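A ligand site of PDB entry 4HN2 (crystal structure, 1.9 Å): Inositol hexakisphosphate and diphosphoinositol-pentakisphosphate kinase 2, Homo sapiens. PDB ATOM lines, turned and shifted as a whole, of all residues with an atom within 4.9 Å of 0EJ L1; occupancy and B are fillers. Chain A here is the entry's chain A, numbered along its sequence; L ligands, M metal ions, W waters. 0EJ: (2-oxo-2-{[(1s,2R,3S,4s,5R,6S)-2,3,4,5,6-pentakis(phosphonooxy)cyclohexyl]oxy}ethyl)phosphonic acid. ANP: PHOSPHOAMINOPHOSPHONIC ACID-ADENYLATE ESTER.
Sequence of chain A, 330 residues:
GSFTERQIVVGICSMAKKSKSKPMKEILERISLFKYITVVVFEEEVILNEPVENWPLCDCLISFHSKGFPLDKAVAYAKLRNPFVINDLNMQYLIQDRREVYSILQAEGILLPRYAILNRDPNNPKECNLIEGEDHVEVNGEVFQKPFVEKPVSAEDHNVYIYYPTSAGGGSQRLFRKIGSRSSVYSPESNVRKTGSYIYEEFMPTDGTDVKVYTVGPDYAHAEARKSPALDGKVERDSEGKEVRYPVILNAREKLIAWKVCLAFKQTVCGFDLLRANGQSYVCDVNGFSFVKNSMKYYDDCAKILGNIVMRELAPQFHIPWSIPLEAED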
ATOM      1  N   LYS A  17     -31.533  33.316  -8.102  1.00  0.00           N
ATOM      2  CA  LYS A  17     -30.125  33.537  -7.728  1.00  0.00           C
ATOM      3  C   LYS A  17     -29.152  32.982  -8.770  1.00  0.00           C
ATOM      4  O   LYS A  17     -28.073  33.562  -9.029  1.00  0.00           O
ATOM      5  CB  LYS A  17     -29.889  32.882  -6.366  1.00  0.00           C
ATOM      6  CG  LYS A  17     -28.486  32.975  -5.807  1.00  0.00           C
ATOM      7  CD  LYS A  17     -28.510  32.430  -4.396  1.00  0.00           C
ATOM      8  CE  LYS A  17     -27.174  32.601  -3.731  1.00  0.00           C
ATOM      9  NZ  LYS A  17     -27.157  31.829  -2.449  1.00  0.00           N
ATOM     10  N   LYS A  18     -29.531  31.851  -9.371  1.00  0.00           N
ATOM     11  CA  LYS A  18     -28.715  31.190 -10.378  1.00  0.00           C
ATOM     12  C   LYS A  18     -29.021  31.683 -11.803  1.00  0.00           C
ATOM     13  O   LYS A  18     -28.088  31.964 -12.559  1.00  0.00           O
ATOM     14  CB  LYS A  18     -28.857  29.670 -10.294  1.00  0.00           C
ATOM     15  CG  LYS A  18     -28.604  29.088  -8.888  1.00  0.00           C
ATOM     16  CD  LYS A  18     -27.188  29.376  -8.376  1.00  0.00           C
ATOM     17  CE  LYS A  18     -26.962  28.719  -7.014  1.00  0.00           C
ATOM     18  NZ  LYS A  18     -25.586  28.930  -6.492  1.00  0.00           N
ATOM     19  N   SER A  66     -30.507  23.825  -6.806  1.00  0.00           N
ATOM     20  CA  SER A  66     -29.727  24.468  -5.764  1.00  0.00           C
ATOM     21  C   SER A  66     -30.669  24.638  -4.571  1.00  0.00           C
ATOM     22  O   SER A  66     -31.854  24.266  -4.664  1.00  0.00           O
ATOM     23  CB  SER A  66     -29.136  25.792  -6.267  1.00  0.00           C
ATOM     24  OG  SER A  66     -30.125  26.729  -6.625  1.00  0.00           O
ATOM     25  N   HIS A 158     -21.474  21.988   3.948  1.00  0.00           N
ATOM     26  CA  HIS A 158     -20.066  22.286   3.627  1.00  0.00           C
ATOM     27  C   HIS A 158     -19.136  22.341   4.856  1.00  0.00           C
ATOM     28  O   HIS A 158     -17.990  22.792   4.779  1.00  0.00           O
ATOM     29  CB  HIS A 158     -19.996  23.586   2.810  1.00  0.00           C
ATOM     30  CG  HIS A 158     -20.827  23.542   1.569  1.00  0.00           C
ATOM     31  ND1 HIS A 158     -20.568  22.673   0.536  1.00  0.00           N
ATOM     32  CD2 HIS A 158     -21.957  24.205   1.221  1.00  0.00           C
ATOM     33  CE1 HIS A 158     -21.476  22.813  -0.403  1.00  0.00           C
ATOM     34  NE2 HIS A 158     -22.335  23.737  -0.017  1.00  0.00           N
ATOM     35  N   ARG A 177     -18.667  27.296   4.055  1.00  0.00           N
ATOM     36  CA  ARG A 177     -18.941  28.235   2.982  1.00  0.00           C
ATOM     37  C   ARG A 177     -18.319  29.575   3.356  1.00  0.00           C
ATOM     38  O   ARG A 177     -18.480  30.029   4.484  1.00  0.00           O
ATOM     39  CB  ARG A 177     -20.454  28.415   2.785  1.00  0.00           C
ATOM     40  CG  ARG A 177     -21.043  27.595   1.657  1.00  0.00           C
ATOM     41  CD  ARG A 177     -20.803  28.248   0.282  1.00  0.00           C
ATOM     42  NE  ARG A 177     -21.225  27.343  -0.801  1.00  0.00           N
ATOM     43  CZ  ARG A 177     -20.472  26.354  -1.297  1.00  0.00           C
ATOM     44  NH1 ARG A 177     -19.256  26.139  -0.813  1.00  0.00           N
ATOM     45  NH2 ARG A 177     -20.937  25.587  -2.269  1.00  0.00           N
ATOM     46  N   LYS A 178     -17.574  30.172   2.431  1.00  0.00           N
ATOM     47  CA  LYS A 178     -16.841  31.408   2.704  1.00  0.00           C
ATOM     48  C   LYS A 178     -17.686  32.420   3.460  1.00  0.00           C
ATOM     49  O   LYS A 178     -18.818  32.701   3.074  1.00  0.00           O
ATOM     50  CB  LYS A 178     -16.360  32.065   1.405  1.00  0.00           C
ATOM     51  CG  LYS A 178     -14.997  31.632   0.946  1.00  0.00           C
ATOM     52  CD  LYS A 178     -14.534  32.460  -0.255  1.00  0.00           C
ATOM     53  CE  LYS A 178     -15.195  32.017  -1.552  1.00  0.00           C
ATOM     54  NZ  LYS A 178     -14.855  32.949  -2.665  1.00  0.00           N
ATOM     55  N   LYS A 212     -10.145  23.049  -9.559  1.00  0.00           N
ATOM     56  CA  LYS A 212     -11.570  23.046  -9.872  1.00  0.00           C
ATOM     57  C   LYS A 212     -11.712  22.826 -11.367  1.00  0.00           C
ATOM     58  O   LYS A 212     -11.065  23.530 -12.156  1.00  0.00           O
ATOM     59  CB  LYS A 212     -12.194  24.388  -9.496  1.00  0.00           C
ATOM     60  CG  LYS A 212     -11.912  24.826  -8.070  1.00  0.00           C
ATOM     61  CD  LYS A 212     -12.915  24.219  -7.104  1.00  0.00           C
ATOM     62  CE  LYS A 212     -14.272  24.935  -7.184  1.00  0.00           C
ATOM     63  NZ  LYS A 212     -15.274  24.196  -6.345  1.00  0.00           N
ATOM     64  N   TYR A 214     -14.373  22.395 -14.734  1.00  0.00           N
ATOM     65  CA  TYR A 214     -15.696  22.749 -15.206  1.00  0.00           C
ATOM     66  C   TYR A 214     -15.878  22.180 -16.599  1.00  0.00           C
ATOM     67  O   TYR A 214     -15.175  22.595 -17.536  1.00  0.00           O
ATOM     68  CB  TYR A 214     -15.846  24.268 -15.280  1.00  0.00           C
ATOM     69  CG  TYR A 214     -15.640  24.982 -13.971  1.00  0.00           C
ATOM     70  CD1 TYR A 214     -14.369  25.311 -13.535  1.00  0.00           C
ATOM     71  CD2 TYR A 214     -16.730  25.339 -13.164  1.00  0.00           C
ATOM     72  CE1 TYR A 214     -14.170  25.989 -12.324  1.00  0.00           C
ATOM     73  CE2 TYR A 214     -16.540  26.021 -11.943  1.00  0.00           C
ATOM     74  CZ  TYR A 214     -15.253  26.350 -11.545  1.00  0.00           C
ATOM     75  OH  TYR A 214     -15.024  27.011 -10.348  1.00  0.00           O
ATOM     76  N   GLU A 243     -11.602  36.282  -5.632  1.00  0.00           N
ATOM     77  CA  GLU A 243     -10.696  35.239  -5.141  1.00  0.00           C
ATOM     78  C   GLU A 243      -9.614  34.968  -6.187  1.00  0.00           C
ATOM     79  O   GLU A 243      -9.920  34.902  -7.379  1.00  0.00           O
ATOM     80  CB  GLU A 243     -11.413  33.946  -4.732  1.00  0.00           C
ATOM     81  CG  GLU A 243     -10.501  33.000  -3.926  1.00  0.00           C
ATOM     82  CD  GLU A 243     -11.148  31.708  -3.434  1.00  0.00           C
ATOM     83  OE1 GLU A 243     -12.370  31.508  -3.592  1.00  0.00           O
ATOM     84  OE2 GLU A 243     -10.409  30.869  -2.877  1.00  0.00           O
ATOM     85  N   ARG A 245      -7.272  33.043  -8.523  1.00  0.00           N
ATOM     86  CA  ARG A 245      -7.281  31.761  -9.223  1.00  0.00           C
ATOM     87  C   ARG A 245      -5.923  31.564  -9.922  1.00  0.00           C
ATOM     88  O   ARG A 245      -5.279  32.539 -10.314  1.00  0.00           O
ATOM     89  CB  ARG A 245      -8.446  31.680 -10.237  1.00  0.00           C
ATOM     90  CG  ARG A 245      -9.868  31.793  -9.649  1.00  0.00           C
ATOM     91  CD  ARG A 245     -10.203  30.642  -8.697  1.00  0.00           C
ATOM     92  NE  ARG A 245     -11.551  30.708  -8.125  1.00  0.00           N
ATOM     93  CZ  ARG A 245     -12.104  29.734  -7.399  1.00  0.00           C
ATOM     94  NH1 ARG A 245     -11.425  28.635  -7.159  1.00  0.00           N
ATOM     95  NH2 ARG A 245     -13.338  29.860  -6.914  1.00  0.00           N
ATOM     96  N   ASN A 287     -19.907  18.544  -7.996  1.00  0.00           N
ATOM     97  CA  ASN A 287     -20.942  19.536  -7.656  1.00  0.00           C
ATOM     98  C   ASN A 287     -22.122  19.640  -8.621  1.00  0.00           C
ATOM     99  O   ASN A 287     -23.152  20.230  -8.280  1.00  0.00           O
ATOM    100  CB  ASN A 287     -20.313  20.921  -7.443  1.00  0.00           C
ATOM    101  CG  ASN A 287     -19.309  20.933  -6.308  1.00  0.00           C
ATOM    102  OD1 ASN A 287     -18.208  21.466  -6.433  1.00  0.00           O
ATOM    103  ND2 ASN A 287     -19.683  20.319  -5.183  1.00  0.00           N
ATOM    104  N   PHE A 289     -24.093  21.178 -11.890  1.00  0.00           N
ATOM    105  CA  PHE A 289     -24.145  22.382 -12.718  1.00  0.00           C
ATOM    106  C   PHE A 289     -23.393  23.546 -12.105  1.00  0.00           C
ATOM    107  O   PHE A 289     -23.719  24.003 -10.998  1.00  0.00           O
ATOM    108  CB  PHE A 289     -25.596  22.798 -13.021  1.00  0.00           C
ATOM    109  CG  PHE A 289     -25.719  23.743 -14.178  1.00  0.00           C
ATOM    110  CD1 PHE A 289     -25.398  25.094 -14.028  1.00  0.00           C
ATOM    111  CD2 PHE A 289     -26.158  23.290 -15.412  1.00  0.00           C
ATOM    112  CE1 PHE A 289     -25.525  25.984 -15.106  1.00  0.00           C
ATOM    113  CE2 PHE A 289     -26.285  24.160 -16.500  1.00  0.00           C
ATOM    114  CZ  PHE A 289     -25.963  25.517 -16.342  1.00  0.00           C
ATOM    115  N   SER A 290     -22.389  24.031 -12.829  1.00  0.00           N
ATOM    116  CA  SER A 290     -21.538  25.087 -12.337  1.00  0.00           C
ATOM    117  C   SER A 290     -20.830  25.740 -13.516  1.00  0.00           C
ATOM    118  O   SER A 290     -20.297  25.052 -14.380  1.00  0.00           O
ATOM    119  CB  SER A 290     -20.517  24.546 -11.339  1.00  0.00           C
ATOM    120  OG  SER A 290     -19.818  25.628 -10.737  1.00  0.00           O
ATOM    121  N   PHE A 291     -20.875  27.072 -13.565  1.00  0.00           N
ATOM    122  CA  PHE A 291     -20.153  27.843 -14.607  1.00  0.00           C
ATOM    123  C   PHE A 291     -18.856  28.410 -14.063  1.00  0.00           C
ATOM    124  O   PHE A 291     -18.750  28.729 -12.867  1.00  0.00           O
ATOM    125  CB  PHE A 291     -20.994  29.028 -15.095  1.00  0.00           C
ATOM    126  CG  PHE A 291     -22.164  28.670 -15.988  1.00  0.00           C
ATOM    127  CD1 PHE A 291     -22.065  27.682 -16.950  1.00  0.00           C
ATOM    128  CD2 PHE A 291     -23.352  29.406 -15.900  1.00  0.00           C
ATOM    129  CE1 PHE A 291     -23.146  27.390 -17.796  1.00  0.00           C
ATOM    130  CE2 PHE A 291     -24.433  29.133 -16.736  1.00  0.00           C
ATOM    131  CZ  PHE A 291     -24.331  28.123 -17.694  1.00  0.00           C
ATOM    132  N   LYS A 293     -16.499  31.526 -13.519  1.00  0.00           N
ATOM    133  CA  LYS A 293     -16.736  32.951 -13.306  1.00  0.00           C
ATOM    134  C   LYS A 293     -15.539  33.789 -13.776  1.00  0.00           C
ATOM    135  O   LYS A 293     -14.383  33.371 -13.651  1.00  0.00           O
ATOM    136  CB  LYS A 293     -17.024  33.209 -11.813  1.00  0.00           C
ATOM    137  CG  LYS A 293     -18.367  32.630 -11.295  1.00  0.00           C
ATOM    138  CD  LYS A 293     -18.202  31.226 -10.733  1.00  0.00           C
ATOM    139  CE  LYS A 293     -19.489  30.684 -10.144  1.00  0.00           C
ATOM    140  NZ  LYS A 293     -19.386  29.215  -9.906  1.00  0.00           N
HETATM  141  C1  0EJ L   1     -19.879  27.839  -5.551  1.00  0.00           C
HETATM  142  C2  0EJ L   1     -21.384  27.756  -5.763  1.00  0.00           C
HETATM  143  C3  0EJ L   1     -22.075  28.420  -4.550  1.00  0.00           C
HETATM  144  C4  0EJ L   1     -21.694  29.893  -4.456  1.00  0.00           C
HETATM  145  C5  0EJ L   1     -20.174  30.076  -4.369  1.00  0.00           C
HETATM  146  C6  0EJ L   1     -19.419  29.309  -5.482  1.00  0.00           C
HETATM  147  O11 0EJ L   1     -19.176  27.139  -6.612  1.00  0.00           O
HETATM  148  O12 0EJ L   1     -21.767  28.415  -6.997  1.00  0.00           O
HETATM  149  O13 0EJ L   1     -23.487  28.325  -4.668  1.00  0.00           O
HETATM  150  O14 0EJ L   1     -22.295  30.429  -3.287  1.00  0.00           O
HETATM  151  O15 0EJ L   1     -19.868  31.483  -4.461  1.00  0.00           O
HETATM  152  O16 0EJ L   1     -18.035  29.315  -5.171  1.00  0.00           O
HETATM  153  O21 0EJ L   1     -18.157  25.399  -4.900  1.00  0.00           O
HETATM  154  O22 0EJ L   1     -23.872  27.271  -7.893  1.00  0.00           O
HETATM  155  O23 0EJ L   1     -24.071  28.138  -2.168  1.00  0.00           O
HETATM  156  O24 0EJ L   1     -24.799  31.086  -3.271  1.00  0.00           O
HETATM  157  O25 0EJ L   1     -19.041  31.373  -2.291  1.00  0.00           O
HETATM  158  O26 0EJ L   1     -15.861  30.622  -5.074  1.00  0.00           O
HETATM  159  O31 0EJ L   1     -20.125  24.714  -6.422  1.00  0.00           O
HETATM  160  O32 0EJ L   1     -21.621  26.100  -8.227  1.00  0.00           O
HETATM  161  O33 0EJ L   1     -23.649  26.002  -3.554  1.00  0.00           O
HETATM  162  O34 0EJ L   1     -23.171  32.357  -4.820  1.00  0.00           O
HETATM  163  O36 0EJ L   1     -17.712  31.356  -6.741  1.00  0.00           O
HETATM  164  O41 0EJ L   1     -17.771  25.135  -7.443  1.00  0.00           O
HETATM  165  O42 0EJ L   1     -22.058  28.242  -9.523  1.00  0.00           O
HETATM  166  O43 0EJ L   1     -25.799  27.448  -3.981  1.00  0.00           O
HETATM  167  O44 0EJ L   1     -23.009  32.694  -2.275  1.00  0.00           O
HETATM  168  O45 0EJ L   1     -17.649  35.537  -4.268  1.00  0.00           O
HETATM  169  O46 0EJ L   1     -16.375  29.158  -7.136  1.00  0.00           O
HETATM  170  O55 0EJ L   1     -16.808  33.092  -4.385  1.00  0.00           O
HETATM  171  O65 0EJ L   1     -18.680  33.832  -5.955  1.00  0.00           O
HETATM  172  PA1 0EJ L   1     -18.741  25.570  -6.411  1.00  0.00           P
HETATM  173  PA2 0EJ L   1     -22.304  27.552  -8.245  1.00  0.00           P
HETATM  174  PA3 0EJ L   1     -24.358  27.459  -3.612  1.00  0.00           P
HETATM  175  PA4 0EJ L   1     -23.308  31.712  -3.342  1.00  0.00           P
HETATM  176  CA5 0EJ L   1     -19.383  32.020  -3.279  1.00  0.00           C
HETATM  177  PA6 0EJ L   1     -16.954  30.056  -6.114  1.00  0.00           P
HETATM  178  CB5 0EJ L   1     -19.282  33.539  -3.286  1.00  0.00           C
HETATM  179  PB5 0EJ L   1     -18.123  34.011  -4.594  1.00  0.00           P
HETATM  180  PG  ANP L   2     -17.677  22.808  -2.641  1.00  0.00           P
HETATM  181  O1G ANP L   2     -16.605  22.795  -3.694  1.00  0.00           O
HETATM  182  O2G ANP L   2     -18.052  24.195  -2.170  1.00  0.00           O
HETATM  183  O3G ANP L   2     -18.888  21.960  -2.977  1.00  0.00           O
HETATM  184  PB  ANP L   2     -17.575  20.785  -0.297  1.00  0.00           P
HETATM  185  O1B ANP L   2     -18.263  21.218   0.978  1.00  0.00           O
HETATM  186  O2B ANP L   2     -18.359  19.863  -1.204  1.00  0.00           O
HETATM  187  N3B ANP L   2     -16.913  22.114  -1.219  1.00  0.00           N
HETATM  188  PA  ANP L   2     -15.144  19.256  -0.481  1.00  0.00           P
HETATM  189  O1A ANP L   2     -15.254  17.741  -0.551  1.00  0.00           O
HETATM  190  O2A ANP L   2     -14.833  20.021  -1.742  1.00  0.00           O
HETATM  191  O3A ANP L   2     -16.378  19.889   0.312  1.00  0.00           O
HETATM  192  O5' ANP L   2     -13.973  19.597   0.575  1.00  0.00           O
HETATM  193  C5' ANP L   2     -13.614  20.956   0.793  1.00  0.00           C
HETATM  194  C4' ANP L   2     -12.128  21.141   0.604  1.00  0.00           C
HETATM  195  O4' ANP L   2     -11.436  20.312   1.543  1.00  0.00           O
HETATM  196  C3' ANP L   2     -11.612  20.712  -0.755  1.00  0.00           C
HETATM  197  O3' ANP L   2     -11.641  21.814  -1.658  1.00  0.00           O
HETATM  198  C2' ANP L   2     -10.191  20.273  -0.473  1.00  0.00           C
HETATM  199  O2' ANP L   2      -9.311  21.412  -0.420  1.00  0.00           O
HETATM  200  C1' ANP L   2     -10.259  19.754   0.934  1.00  0.00           C
HETATM  201  N9  ANP L   2     -10.366  18.279   0.933  1.00  0.00           N
HETATM  202  C8  ANP L   2     -11.490  17.540   0.838  1.00  0.00           C
HETATM  203  N7  ANP L   2     -11.205  16.207   0.855  1.00  0.00           N
HETATM  204  C5  ANP L   2      -9.863  16.103   0.963  1.00  0.00           C
HETATM  205  C6  ANP L   2      -8.907  14.990   1.042  1.00  0.00           C
HETATM  206  N6  ANP L   2      -9.377  13.724   0.996  1.00  0.00           N
HETATM  207  N1  ANP L   2      -7.590  15.286   1.150  1.00  0.00           N
HETATM  208  C2  ANP L   2      -7.145  16.562   1.165  1.00  0.00           C
HETATM  209  N3  ANP L   2      -7.971  17.633   1.113  1.00  0.00           N
HETATM  210  C4  ANP L   2      -9.312  17.457   1.003  1.00  0.00           C
HETATM  211 MG    MG M   1     -24.633  23.276  -6.590  1.00  0.00          MG
HETATM  212  O   HOH W   1     -24.498  25.353  -5.941  1.00  0.00           O
HETATM  213  O   HOH W   2     -17.937  23.146  -9.033  1.00  0.00           O
HETATM  214  O   HOH W   3     -24.244  23.624  -2.296  1.00  0.00           O
HETATM  215  O   HOH W   4     -25.216  31.569  -6.324  1.00  0.00           O
HETATM  216  O   HOH W   5     -24.122  26.436   0.054  1.00  0.00           O
HETATM  217  O   HOH W   6     -23.240  23.624  -8.263  1.00  0.00           O
HETATM  218  O   HOH W   7     -27.133  25.166  -3.309  1.00  0.00           O
HETATM  219  O   HOH W   8     -22.637  28.580 -11.861  1.00  0.00           O
HETATM  220  O   HOH W   9     -17.249  27.453  -8.865  1.00  0.00           O
HETATM  221  O   HOH W  10     -27.729  28.925  -3.037  1.00  0.00           O
HETATM  222  O   HOH W  11     -25.469  25.854  -9.465  1.00  0.00           O
HETATM  223  O   HOH W  12     -21.227  23.375  -4.175  1.00  0.00           O
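A ring nitrogen (ND1) of His 158 lies within hydrogen-bond range of an oxygen (O1B) of ANP L2 (2.8 Å). The guanidinium group (NH2) of Arg 177 is in salt-bridge range of an oxygen (O33) of 0EJ L1 (3.0 Å). An oxygen (O1G) of ANP L2 lies close to the side-chain amino group (NZ) of Lys 212, 3.3 Å away. The side-chain hydroxyl (OG) of Ser 290 is in hydrogen-bond range of an oxygen (O32) of 0EJ L1, at 3.1 Å. NH2 of Arg 245 is in salt-bridge range of O46 of 0EJ L1 (3.1 Å). The side-chain amino group (NZ) of Lys 212 lies within salt-bridge range of an oxygen (O41) of 0EJ L1 (2.9 Å). An oxygen (O42) of 0EJ L1 is in salt-bridge range of the side-chain amino group (NZ) of Lys 293 (2.9 Å). O22 of 0EJ L1 lies within salt-bridge range of NZ of Lys 18 (2.8 Å). O2G of ANP L2 lies within salt-bridge range of NH1 of Arg 177 (2.7 Å). NZ of Lys 17 lies within salt-bridge range of O24 of 0EJ L1 (2.6 Å). NZ of Lys 178 is in salt-bridge range of O55 of 0EJ L1, 2.6 Å away.
O21 of 0EJ L1 lies close to O2G of ANP L2 (3.0 Å).
NE2 of His 158 is in hydrogen-bond range of NH2 of Arg 177 (3.2 Å). OE1 of Glu 243 lies within salt-bridge range of NH2 of Arg 245. O of Phe 291 is in hydrogen-bond range of NZ of Lys 293, 3.1 Å away. The side-chain carboxylate (OE1) of Glu 243 lies within salt-bridge range of the side-chain amino group (NZ) of Lys 178 (3.0 Å).
Residues that only touch 0EJ L1: Asn 287 and Glu 243. Within 4 Å of 0EJ L1: Lys 17, Lys 18, Arg 177, Lys 178, Lys 212, Glu 243, Arg 245, Asn 287, Ser 290 and Lys 293.
Water W8 bridges O42 of 0EJ L1 (2.4 Å) and N of Phe 291 (2.9 Å). Water W2 lies within hydrogen-bond range of O41 of 0EJ L1 (2.6 Å) and OD1 of Asn 287 (3.1 Å). Water W4 lies within hydrogen-bond range of O34 of 0EJ L1 (2.7 Å) and NZ of Lys 18 (2.7 Å). Water W3 lies within hydrogen-bond range of O33 of 0EJ L1 (2.8 Å) and NE2 of His 158 (3.0 Å). Water W5 lies within hydrogen-bond range of an oxygen (O23) of 0EJ L1, the guanidinium group (NE) of Arg 177 and a ring nitrogen (NE2) of His 158. Water W12 lies within hydrogen-bond range of O31 of 0EJ L1 and NH2 of Arg 177.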
